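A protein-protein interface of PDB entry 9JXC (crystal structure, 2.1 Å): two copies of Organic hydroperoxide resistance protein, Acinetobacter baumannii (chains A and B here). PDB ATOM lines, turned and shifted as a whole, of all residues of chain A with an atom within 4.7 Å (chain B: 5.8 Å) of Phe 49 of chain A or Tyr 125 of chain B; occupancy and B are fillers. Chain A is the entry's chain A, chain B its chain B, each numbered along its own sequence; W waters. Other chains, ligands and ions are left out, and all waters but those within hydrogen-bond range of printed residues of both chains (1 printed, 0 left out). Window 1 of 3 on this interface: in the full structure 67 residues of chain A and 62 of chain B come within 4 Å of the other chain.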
ATOM      1  N   PRO A  45       6.906 -32.586  10.341  1.00  0.00           N
ATOM      2  CA  PRO A  45       8.169 -31.911  10.654  1.00  0.00           C
ATOM      3  C   PRO A  45       8.643 -30.902   9.603  1.00  0.00           C
ATOM      4  O   PRO A  45       9.298 -29.943   9.978  1.00  0.00           O
ATOM      5  CB  PRO A  45       9.147 -33.098  10.806  1.00  0.00           C
ATOM      6  CG  PRO A  45       8.229 -34.240  11.289  1.00  0.00           C
ATOM      7  CD  PRO A  45       7.015 -34.054  10.409  1.00  0.00           C
ATOM      8  N   GLU A  46       8.312 -31.102   8.327  1.00  0.00           N
ATOM      9  CA  GLU A  46       8.773 -30.172   7.265  1.00  0.00           C
ATOM     10  C   GLU A  46       8.019 -28.871   7.473  1.00  0.00           C
ATOM     11  O   GLU A  46       8.646 -27.834   7.467  1.00  0.00           O
ATOM     12  CB  GLU A  46       8.635 -30.741   5.846  1.00  0.00           C
ATOM     13  CG  GLU A  46       9.593 -31.900   5.589  1.00  0.00           C
ATOM     14  CD  GLU A  46       9.247 -33.174   6.341  1.00  0.00           C
ATOM     15  OE1 GLU A  46      10.180 -33.880   6.741  1.00  0.00           O
ATOM     16  OE2 GLU A  46       8.039 -33.456   6.535  1.00  0.00           O
ATOM     17  N   GLN A  47       6.710 -28.945   7.685  1.00  0.00           N
ATOM     18  CA  GLN A  47       5.865 -27.745   7.835  1.00  0.00           C
ATOM     19  C   GLN A  47       6.234 -27.011   9.127  1.00  0.00           C
ATOM     20  O   GLN A  47       6.280 -25.780   9.083  1.00  0.00           O
ATOM     21  CB  GLN A  47       4.400 -28.170   7.747  1.00  0.00           C
ATOM     22  CG  GLN A  47       3.441 -27.021   7.554  1.00  0.00           C
ATOM     23  CD  GLN A  47       2.043 -27.579   7.446  1.00  0.00           C
ATOM     24  OE1 GLN A  47       1.527 -28.131   8.413  1.00  0.00           O
ATOM     25  NE2 GLN A  47       1.524 -27.570   6.233  1.00  0.00           N
ATOM     26  N   LEU A  48       6.491 -27.721  10.236  1.00  0.00           N
ATOM     27  CA  LEU A  48       6.934 -27.082  11.508  1.00  0.00           C
ATOM     28  C   LEU A  48       8.275 -26.352  11.291  1.00  0.00           C
ATOM     29  O   LEU A  48       8.470 -25.222  11.808  1.00  0.00           O
ATOM     30  CB  LEU A  48       7.007 -28.133  12.634  1.00  0.00           C
ATOM     31  CG  LEU A  48       5.645 -28.654  13.083  1.00  0.00           C
ATOM     32  CD1 LEU A  48       5.764 -29.928  13.881  1.00  0.00           C
ATOM     33  CD2 LEU A  48       4.870 -27.581  13.845  1.00  0.00           C
ATOM     34  N   PHE A  49       9.207 -26.944  10.576  1.00  0.00           N
ATOM     35  CA  PHE A  49      10.532 -26.294  10.351  1.00  0.00           C
ATOM     36  C   PHE A  49      10.346 -25.057   9.465  1.00  0.00           C
ATOM     37  O   PHE A  49      10.982 -24.058   9.697  1.00  0.00           O
ATOM     38  CB  PHE A  49      11.516 -27.267   9.711  1.00  0.00           C
ATOM     39  CG  PHE A  49      12.916 -26.719   9.601  1.00  0.00           C
ATOM     40  CD1 PHE A  49      13.790 -26.779  10.673  1.00  0.00           C
ATOM     41  CD2 PHE A  49      13.370 -26.159   8.421  1.00  0.00           C
ATOM     42  CE1 PHE A  49      15.084 -26.281  10.555  1.00  0.00           C
ATOM     43  CE2 PHE A  49      14.658 -25.659   8.313  1.00  0.00           C
ATOM     44  CZ  PHE A  49      15.501 -25.706   9.387  1.00  0.00           C
ATOM     45  N   ALA A  50       9.529 -25.146   8.426  1.00  0.00           N
ATOM     46  CA  ALA A  50       9.253 -24.012   7.510  1.00  0.00           C
ATOM     47  C   ALA A  50       8.645 -22.868   8.338  1.00  0.00           C
ATOM     48  O   ALA A  50       9.078 -21.705   8.146  1.00  0.00           O
ATOM     49  CB  ALA A  50       8.384 -24.470   6.369  1.00  0.00           C
ATOM     50  N   ALA A  51       7.762 -23.200   9.297  1.00  0.00           N
ATOM     51  CA  ALA A  51       7.069 -22.205  10.139  1.00  0.00           C
ATOM     52  C   ALA A  51       8.093 -21.572  11.094  1.00  0.00           C
ATOM     53  O   ALA A  51       8.164 -20.357  11.153  1.00  0.00           O
ATOM     54  CB  ALA A  51       5.900 -22.819  10.869  1.00  0.00           C
ATOM     55  N   GLY A  52       8.912 -22.375  11.755  1.00  0.00           N
ATOM     56  CA  GLY A  52       9.915 -21.863  12.704  1.00  0.00           C
ATOM     57  C   GLY A  52      10.922 -20.958  12.017  1.00  0.00           C
ATOM     58  O   GLY A  52      11.200 -19.849  12.534  1.00  0.00           O
ATOM     59  N   TYR A  53      11.427 -21.384  10.856  1.00  0.00           N
ATOM     60  CA  TYR A  53      12.463 -20.658  10.085  1.00  0.00           C
ATOM     61  C   TYR A  53      11.890 -19.336   9.546  1.00  0.00           C
ATOM     62  O   TYR A  53      12.526 -18.249   9.656  1.00  0.00           O
ATOM     63  CB  TYR A  53      12.990 -21.545   8.946  1.00  0.00           C
ATOM     64  CG  TYR A  53      14.363 -21.188   8.417  1.00  0.00           C
ATOM     65  CD1 TYR A  53      14.994 -19.992   8.747  1.00  0.00           C
ATOM     66  CD2 TYR A  53      15.008 -22.021   7.521  1.00  0.00           C
ATOM     67  CE1 TYR A  53      16.259 -19.686   8.283  1.00  0.00           C
ATOM     68  CE2 TYR A  53      16.258 -21.700   7.008  1.00  0.00           C
ATOM     69  CZ  TYR A  53      16.896 -20.542   7.408  1.00  0.00           C
ATOM     70  OH  TYR A  53      18.122 -20.215   6.897  1.00  0.00           O
ATOM     71  N   VAL A  84      10.155 -25.808   2.418  1.00  0.00           N
ATOM     72  CA  VAL A  84      10.965 -26.895   3.019  1.00  0.00           C
ATOM     73  C   VAL A  84      10.551 -28.217   2.381  1.00  0.00           C
ATOM     74  O   VAL A  84       9.347 -28.541   2.434  1.00  0.00           O
ATOM     75  CB  VAL A  84      10.812 -26.873   4.543  1.00  0.00           C
ATOM     76  CG1 VAL A  84      11.467 -28.078   5.193  1.00  0.00           C
ATOM     77  CG2 VAL A  84      11.375 -25.566   5.086  1.00  0.00           C
ATOM     78  N   LEU A  96      16.792 -32.029   4.731  1.00  0.00           N
ATOM     79  CA  LEU A  96      15.880 -30.921   4.380  1.00  0.00           C
ATOM     80  C   LEU A  96      16.521 -30.097   3.290  1.00  0.00           C
ATOM     81  O   LEU A  96      17.751 -29.960   3.282  1.00  0.00           O
ATOM     82  CB  LEU A  96      15.578 -30.034   5.586  1.00  0.00           C
ATOM     83  CG  LEU A  96      14.990 -30.751   6.805  1.00  0.00           C
ATOM     84  CD1 LEU A  96      14.689 -29.746   7.895  1.00  0.00           C
ATOM     85  CD2 LEU A  96      13.749 -31.521   6.441  1.00  0.00           C
ATOM     86  N   VAL A  98      15.846 -26.046   1.869  1.00  0.00           N
ATOM     87  CA  VAL A  98      15.216 -24.777   2.331  1.00  0.00           C
ATOM     88  C   VAL A  98      15.440 -23.706   1.282  1.00  0.00           C
ATOM     89  O   VAL A  98      16.563 -23.478   0.902  1.00  0.00           O
ATOM     90  CB  VAL A  98      15.701 -24.294   3.712  1.00  0.00           C
ATOM     91  CG1 VAL A  98      14.850 -23.121   4.174  1.00  0.00           C
ATOM     92  CG2 VAL A  98      15.648 -25.382   4.763  1.00  0.00           C
ATOM     93  N   TYR A 125      18.438 -20.030  13.099  1.00  0.00           N
ATOM     94  CA  TYR A 125      18.134 -21.190  12.199  1.00  0.00           C
ATOM     95  C   TYR A 125      19.177 -21.283  11.077  1.00  0.00           C
ATOM     96  O   TYR A 125      19.677 -22.388  10.788  1.00  0.00           O
ATOM     97  CB  TYR A 125      16.746 -21.050  11.601  1.00  0.00           C
ATOM     98  CG  TYR A 125      15.621 -21.653  12.397  1.00  0.00           C
ATOM     99  CD1 TYR A 125      15.286 -21.186  13.656  1.00  0.00           C
ATOM    100  CD2 TYR A 125      14.793 -22.607  11.815  1.00  0.00           C
ATOM    101  CE1 TYR A 125      14.194 -21.682  14.338  1.00  0.00           C
ATOM    102  CE2 TYR A 125      13.687 -23.111  12.473  1.00  0.00           C
ATOM    103  CZ  TYR A 125      13.388 -22.645  13.738  1.00  0.00           C
ATOM    104  OH  TYR A 125      12.282 -23.157  14.349  1.00  0.00           O
ATOM    105  N   ILE A 129      22.132 -24.474  10.530  1.00  0.00           N
ATOM    106  CA  ILE A 129      22.161 -25.426   9.384  1.00  0.00           C
ATOM    107  C   ILE A 129      23.340 -25.158   8.431  1.00  0.00           C
ATOM    108  O   ILE A 129      23.476 -25.965   7.496  1.00  0.00           O
ATOM    109  CB  ILE A 129      20.793 -25.435   8.668  1.00  0.00           C
ATOM    110  CG1 ILE A 129      20.493 -24.152   7.874  1.00  0.00           C
ATOM    111  CG2 ILE A 129      19.724 -25.751   9.679  1.00  0.00           C
ATOM    112  CD1 ILE A 129      19.112 -24.150   7.222  1.00  0.00           C
ATOM    113  N   LEU B  48       8.404 -24.310  17.871  1.00  0.00           N
ATOM    114  CA  LEU B  48       8.105 -24.949  16.564  1.00  0.00           C
ATOM    115  C   LEU B  48       9.238 -25.898  16.203  1.00  0.00           C
ATOM    116  O   LEU B  48       8.953 -27.022  15.716  1.00  0.00           O
ATOM    117  CB  LEU B  48       7.869 -23.863  15.501  1.00  0.00           C
ATOM    118  CG  LEU B  48       6.586 -23.064  15.709  1.00  0.00           C
ATOM    119  CD1 LEU B  48       6.570 -21.820  14.844  1.00  0.00           C
ATOM    120  CD2 LEU B  48       5.348 -23.924  15.432  1.00  0.00           C
ATOM    121  N   PHE B  49      10.482 -25.491  16.462  1.00  0.00           N
ATOM    122  CA  PHE B  49      11.672 -26.343  16.206  1.00  0.00           C
ATOM    123  C   PHE B  49      11.630 -27.587  17.119  1.00  0.00           C
ATOM    124  O   PHE B  49      11.868 -28.739  16.660  1.00  0.00           O
ATOM    125  CB  PHE B  49      12.970 -25.545  16.398  1.00  0.00           C
ATOM    126  CG  PHE B  49      14.192 -26.306  15.960  1.00  0.00           C
ATOM    127  CD1 PHE B  49      14.380 -26.621  14.631  1.00  0.00           C
ATOM    128  CD2 PHE B  49      15.134 -26.735  16.867  1.00  0.00           C
ATOM    129  CE1 PHE B  49      15.487 -27.347  14.223  1.00  0.00           C
ATOM    130  CE2 PHE B  49      16.249 -27.459  16.452  1.00  0.00           C
ATOM    131  CZ  PHE B  49      16.433 -27.740  15.135  1.00  0.00           C
ATOM    132  N   ALA B  51       9.008 -28.953  18.513  1.00  0.00           N
ATOM    133  CA  ALA B  51       7.886 -29.789  18.058  1.00  0.00           C
ATOM    134  C   ALA B  51       8.336 -30.606  16.836  1.00  0.00           C
ATOM    135  O   ALA B  51       8.121 -31.840  16.810  1.00  0.00           O
ATOM    136  CB  ALA B  51       6.701 -28.941  17.718  1.00  0.00           C
ATOM    137  N   GLY B  52       8.888 -29.925  15.831  1.00  0.00           N
ATOM    138  CA  GLY B  52       9.299 -30.607  14.600  1.00  0.00           C
ATOM    139  C   GLY B  52      10.379 -31.629  14.899  1.00  0.00           C
ATOM    140  O   GLY B  52      10.334 -32.726  14.319  1.00  0.00           O
ATOM    141  N   TYR B  53      11.359 -31.276  15.726  1.00  0.00           N
ATOM    142  CA  TYR B  53      12.517 -32.174  15.988  1.00  0.00           C
ATOM    143  C   TYR B  53      12.010 -33.434  16.728  1.00  0.00           C
ATOM    144  O   TYR B  53      12.366 -34.555  16.384  1.00  0.00           O
ATOM    145  CB  TYR B  53      13.625 -31.439  16.748  1.00  0.00           C
ATOM    146  CG  TYR B  53      15.001 -32.053  16.643  1.00  0.00           C
ATOM    147  CD1 TYR B  53      15.222 -33.297  16.073  1.00  0.00           C
ATOM    148  CD2 TYR B  53      16.114 -31.378  17.096  1.00  0.00           C
ATOM    149  CE1 TYR B  53      16.494 -33.862  16.003  1.00  0.00           C
ATOM    150  CE2 TYR B  53      17.393 -31.912  17.000  1.00  0.00           C
ATOM    151  CZ  TYR B  53      17.592 -33.168  16.467  1.00  0.00           C
ATOM    152  OH  TYR B  53      18.870 -33.680  16.347  1.00  0.00           O
ATOM    153  N   CYS B  56      10.074 -35.493  14.215  1.00  0.00           N
ATOM    154  CA  CYS B  56      10.969 -36.000  13.154  1.00  0.00           C
ATOM    155  C   CYS B  56      11.804 -37.161  13.719  1.00  0.00           C
ATOM    156  O   CYS B  56      11.913 -38.200  13.084  1.00  0.00           O
ATOM    157  CB  CYS B  56      11.865 -34.899  12.643  1.00  0.00           C
ATOM    158  SG  CYS B  56      12.820 -35.466  11.232  1.00  0.00           S
ATOM    159  N   CYS B 123      17.573 -39.009  10.823  1.00  0.00           N
ATOM    160  CA  CYS B 123      16.744 -37.828  11.145  1.00  0.00           C
ATOM    161  C   CYS B 123      17.236 -36.589  10.399  1.00  0.00           C
ATOM    162  O   CYS B 123      18.367 -36.135  10.622  1.00  0.00           O
ATOM    163  CB  CYS B 123      16.765 -37.540  12.635  1.00  0.00           C
ATOM    164  SG  CYS B 123      15.717 -36.146  13.059  1.00  0.00           S
ATOM    165  N   PRO B 124      16.409 -35.988   9.509  1.00  0.00           N
ATOM    166  CA  PRO B 124      16.847 -34.831   8.733  1.00  0.00           C
ATOM    167  C   PRO B 124      17.118 -33.607   9.624  1.00  0.00           C
ATOM    168  O   PRO B 124      17.940 -32.824   9.256  1.00  0.00           O
ATOM    169  CB  PRO B 124      15.733 -34.551   7.726  1.00  0.00           C
ATOM    170  CG  PRO B 124      14.548 -35.361   8.194  1.00  0.00           C
ATOM    171  CD  PRO B 124      15.053 -36.405   9.164  1.00  0.00           C
ATOM    172  N   TYR B 125      16.457 -33.476  10.776  1.00  0.00           N
ATOM    173  CA  TYR B 125      16.749 -32.354  11.699  1.00  0.00           C
ATOM    174  C   TYR B 125      18.183 -32.539  12.232  1.00  0.00           C
ATOM    175  O   TYR B 125      18.922 -31.553  12.273  1.00  0.00           O
ATOM    176  CB  TYR B 125      15.738 -32.290  12.841  1.00  0.00           C
ATOM    177  CG  TYR B 125      14.455 -31.545  12.578  1.00  0.00           C
ATOM    178  CD1 TYR B 125      13.635 -31.874  11.518  1.00  0.00           C
ATOM    179  CD2 TYR B 125      14.040 -30.534  13.430  1.00  0.00           C
ATOM    180  CE1 TYR B 125      12.420 -31.228  11.318  1.00  0.00           C
ATOM    181  CE2 TYR B 125      12.849 -29.849  13.220  1.00  0.00           C
ATOM    182  CZ  TYR B 125      12.024 -30.217  12.179  1.00  0.00           C
ATOM    183  OH  TYR B 125      10.836 -29.569  12.008  1.00  0.00           O
ATOM    184  N   SER B 126      18.564 -33.751  12.662  1.00  0.00           N
ATOM    185  CA  SER B 126      19.917 -34.038  13.197  1.00  0.00           C
ATOM    186  C   SER B 126      20.964 -33.742  12.130  1.00  0.00           C
ATOM    187  O   SER B 126      21.961 -33.115  12.475  1.00  0.00           O
ATOM    188  CB  SER B 126      20.058 -35.479  13.700  1.00  0.00           C
ATOM    189  OG  SER B 126      19.110 -35.694  14.722  1.00  0.00           O
ATOM    190  N   ASN B 127      20.739 -34.225  10.902  1.00  0.00           N
ATOM    191  CA  ASN B 127      21.645 -34.023   9.753  1.00  0.00           C
ATOM    192  C   ASN B 127      21.772 -32.507   9.483  1.00  0.00           C
ATOM    193  O   ASN B 127      22.862 -32.067   9.143  1.00  0.00           O
ATOM    194  CB  ASN B 127      21.163 -34.811   8.525  1.00  0.00           C
ATOM    195  CG  ASN B 127      21.430 -36.289   8.702  1.00  0.00           C
ATOM    196  OD1 ASN B 127      22.395 -36.647   9.375  1.00  0.00           O
ATOM    197  ND2 ASN B 127      20.583 -37.146   8.147  1.00  0.00           N
ATOM    198  N   ALA B 128      20.679 -31.759   9.628  1.00  0.00           N
ATOM    199  CA  ALA B 128      20.607 -30.313   9.332  1.00  0.00           C
ATOM    200  C   ALA B 128      21.556 -29.523  10.253  1.00  0.00           C
ATOM    201  O   ALA B 128      22.088 -28.532   9.805  1.00  0.00           O
ATOM    202  CB  ALA B 128      19.180 -29.850   9.551  1.00  0.00           C
ATOM    203  N   ILE B 129      21.642 -29.874  11.537  1.00  0.00           N
ATOM    204  CA  ILE B 129      22.221 -28.978  12.589  1.00  0.00           C
ATOM    205  C   ILE B 129      23.582 -29.514  13.049  1.00  0.00           C
ATOM    206  O   ILE B 129      24.200 -28.849  13.868  1.00  0.00           O
ATOM    207  CB  ILE B 129      21.225 -28.792  13.753  1.00  0.00           C
ATOM    208  CG1 ILE B 129      21.034 -30.092  14.555  1.00  0.00           C
ATOM    209  CG2 ILE B 129      19.910 -28.249  13.196  1.00  0.00           C
ATOM    210  CD1 ILE B 129      19.928 -30.049  15.552  1.00  0.00           C
ATOM    211  N   ARG B 130      23.990 -30.697  12.617  1.00  0.00           N
ATOM    212  CA  ARG B 130      25.261 -31.305  13.091  1.00  0.00           C
ATOM    213  C   ARG B 130      26.429 -30.320  12.940  1.00  0.00           C
ATOM    214  O   ARG B 130      26.548 -29.674  11.885  1.00  0.00           O
ATOM    215  CB  ARG B 130      25.570 -32.594  12.332  1.00  0.00           C
ATOM    216  CG  ARG B 130      26.735 -33.362  12.951  1.00  0.00           C
ATOM    217  CD  ARG B 130      26.815 -34.824  12.542  1.00  0.00           C
ATOM    218  NE  ARG B 130      25.595 -35.555  12.859  1.00  0.00           N
ATOM    219  CZ  ARG B 130      24.744 -36.024  11.954  1.00  0.00           C
ATOM    220  NH1 ARG B 130      24.980 -35.896  10.662  1.00  0.00           N
ATOM    221  NH2 ARG B 130      23.645 -36.635  12.336  1.00  0.00           N
HETATM  222  O   HOH W   1      18.943 -31.961   6.754  1.00  0.00           O
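OH of Tyr 125 of chain B lies within hydrogen-bond range of O of Pro 45 of chain A, at 2.6 Å.
The side-chain hydroxyl (OH) of Tyr 125 of chain B sits close to the backbone NH (N) of Phe 49 of chain A (3.4 Å).
The side-chain sulfur of Cys 56 of chain B is in hydrogen-bond range of the side-chain sulfur of Cys 123 of chain B (3.5 Å).
SG of Cys 123 of chain B sits close to N of Tyr 125 of chain B (3.6 Å).
Among the printed residues, pairs that only touch across the chains: Ile 129 of chain A with Ala 128 of chain B (3.1 Å), Tyr 125 of chain A with Phe 49 of chain B (3.2 Å), Leu 48 of chain A with Gly 52 of chain B (3.7 Å), Pro 45 of chain A with Cys 56 of chain B (3.7 Å), Pro 45 of chain A with Gly 52 of chain B (3.7 Å), Leu 48 of chain A with Leu 48 of chain B (3.8 Å), Phe 49 of chain A with Phe 49 of chain B (3.8 Å), Leu 96 of chain A with Pro 124 of chain B (3.8 Å), Gly 52 of chain A with Leu 48 of chain B (3.9 Å) and Leu 48 of chain A with Ala 51 of chain B (3.98 Å).
Printed residues of chain A within 4 Å of Pro 124 of chain B: Leu 96.
Of the printed residues of chain A, Leu 48 of chain B touches Leu 48 (3.8 Å) and Gly 52 (3.9 Å).
Of the printed residues of chain A, Phe 49 of chain B touches Phe 49 and Tyr 125.
The nearest residue of chain A that does not touch Tyr 125 of chain B is Leu 48 of chain A (4.1 Å).
Of the 14 printed residues of chain B, 8 touch a printed residue of chain A.
Of the 14 printed residues of chain A, 7 touch a printed residue of chain B.
Hydrophobic or aromatic side chains of chain A within 4 Å of the printed part of chain B: Pro 45, Leu 48, Phe 49, Leu 96, Tyr 125 and Ile 129.
Among the printed residues, 12 pairs touch across the chains.
Among the printed residues, no Asp or Glu carboxylate lies within 4 Å of a Lys or Arg side-chain nitrogen of the other chain.
Leu 48 of chain A touches Ala 51 of chain B, but with the chains exchanged Ala 51 of chain A does not touch Leu 48 of chain B (4.1 Å).
Leu 48 of chain A touches Gly 52 of chain B, and with the chains exchanged Gly 52 of chain A touches Leu 48 of chain B.
Phe 49 of chain A touches its own counterpart, Phe 49 of chain B.
Phe 49 of chain A touches Tyr 125 of chain B, and with the chains exchanged Tyr 125 of chain A touches Phe 49 of chain B.
Of the 12 pairs that touch across the chains among the printed residues, 6 have their exchanged pair printed and touching as well.
Water W1 lies within hydrogen-bond range of O of Pro 124 of chain B (2.8 Å), N of Leu 96 of chain A (3.0 Å) and N of Ala 128 of chain B (3.4 Å).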
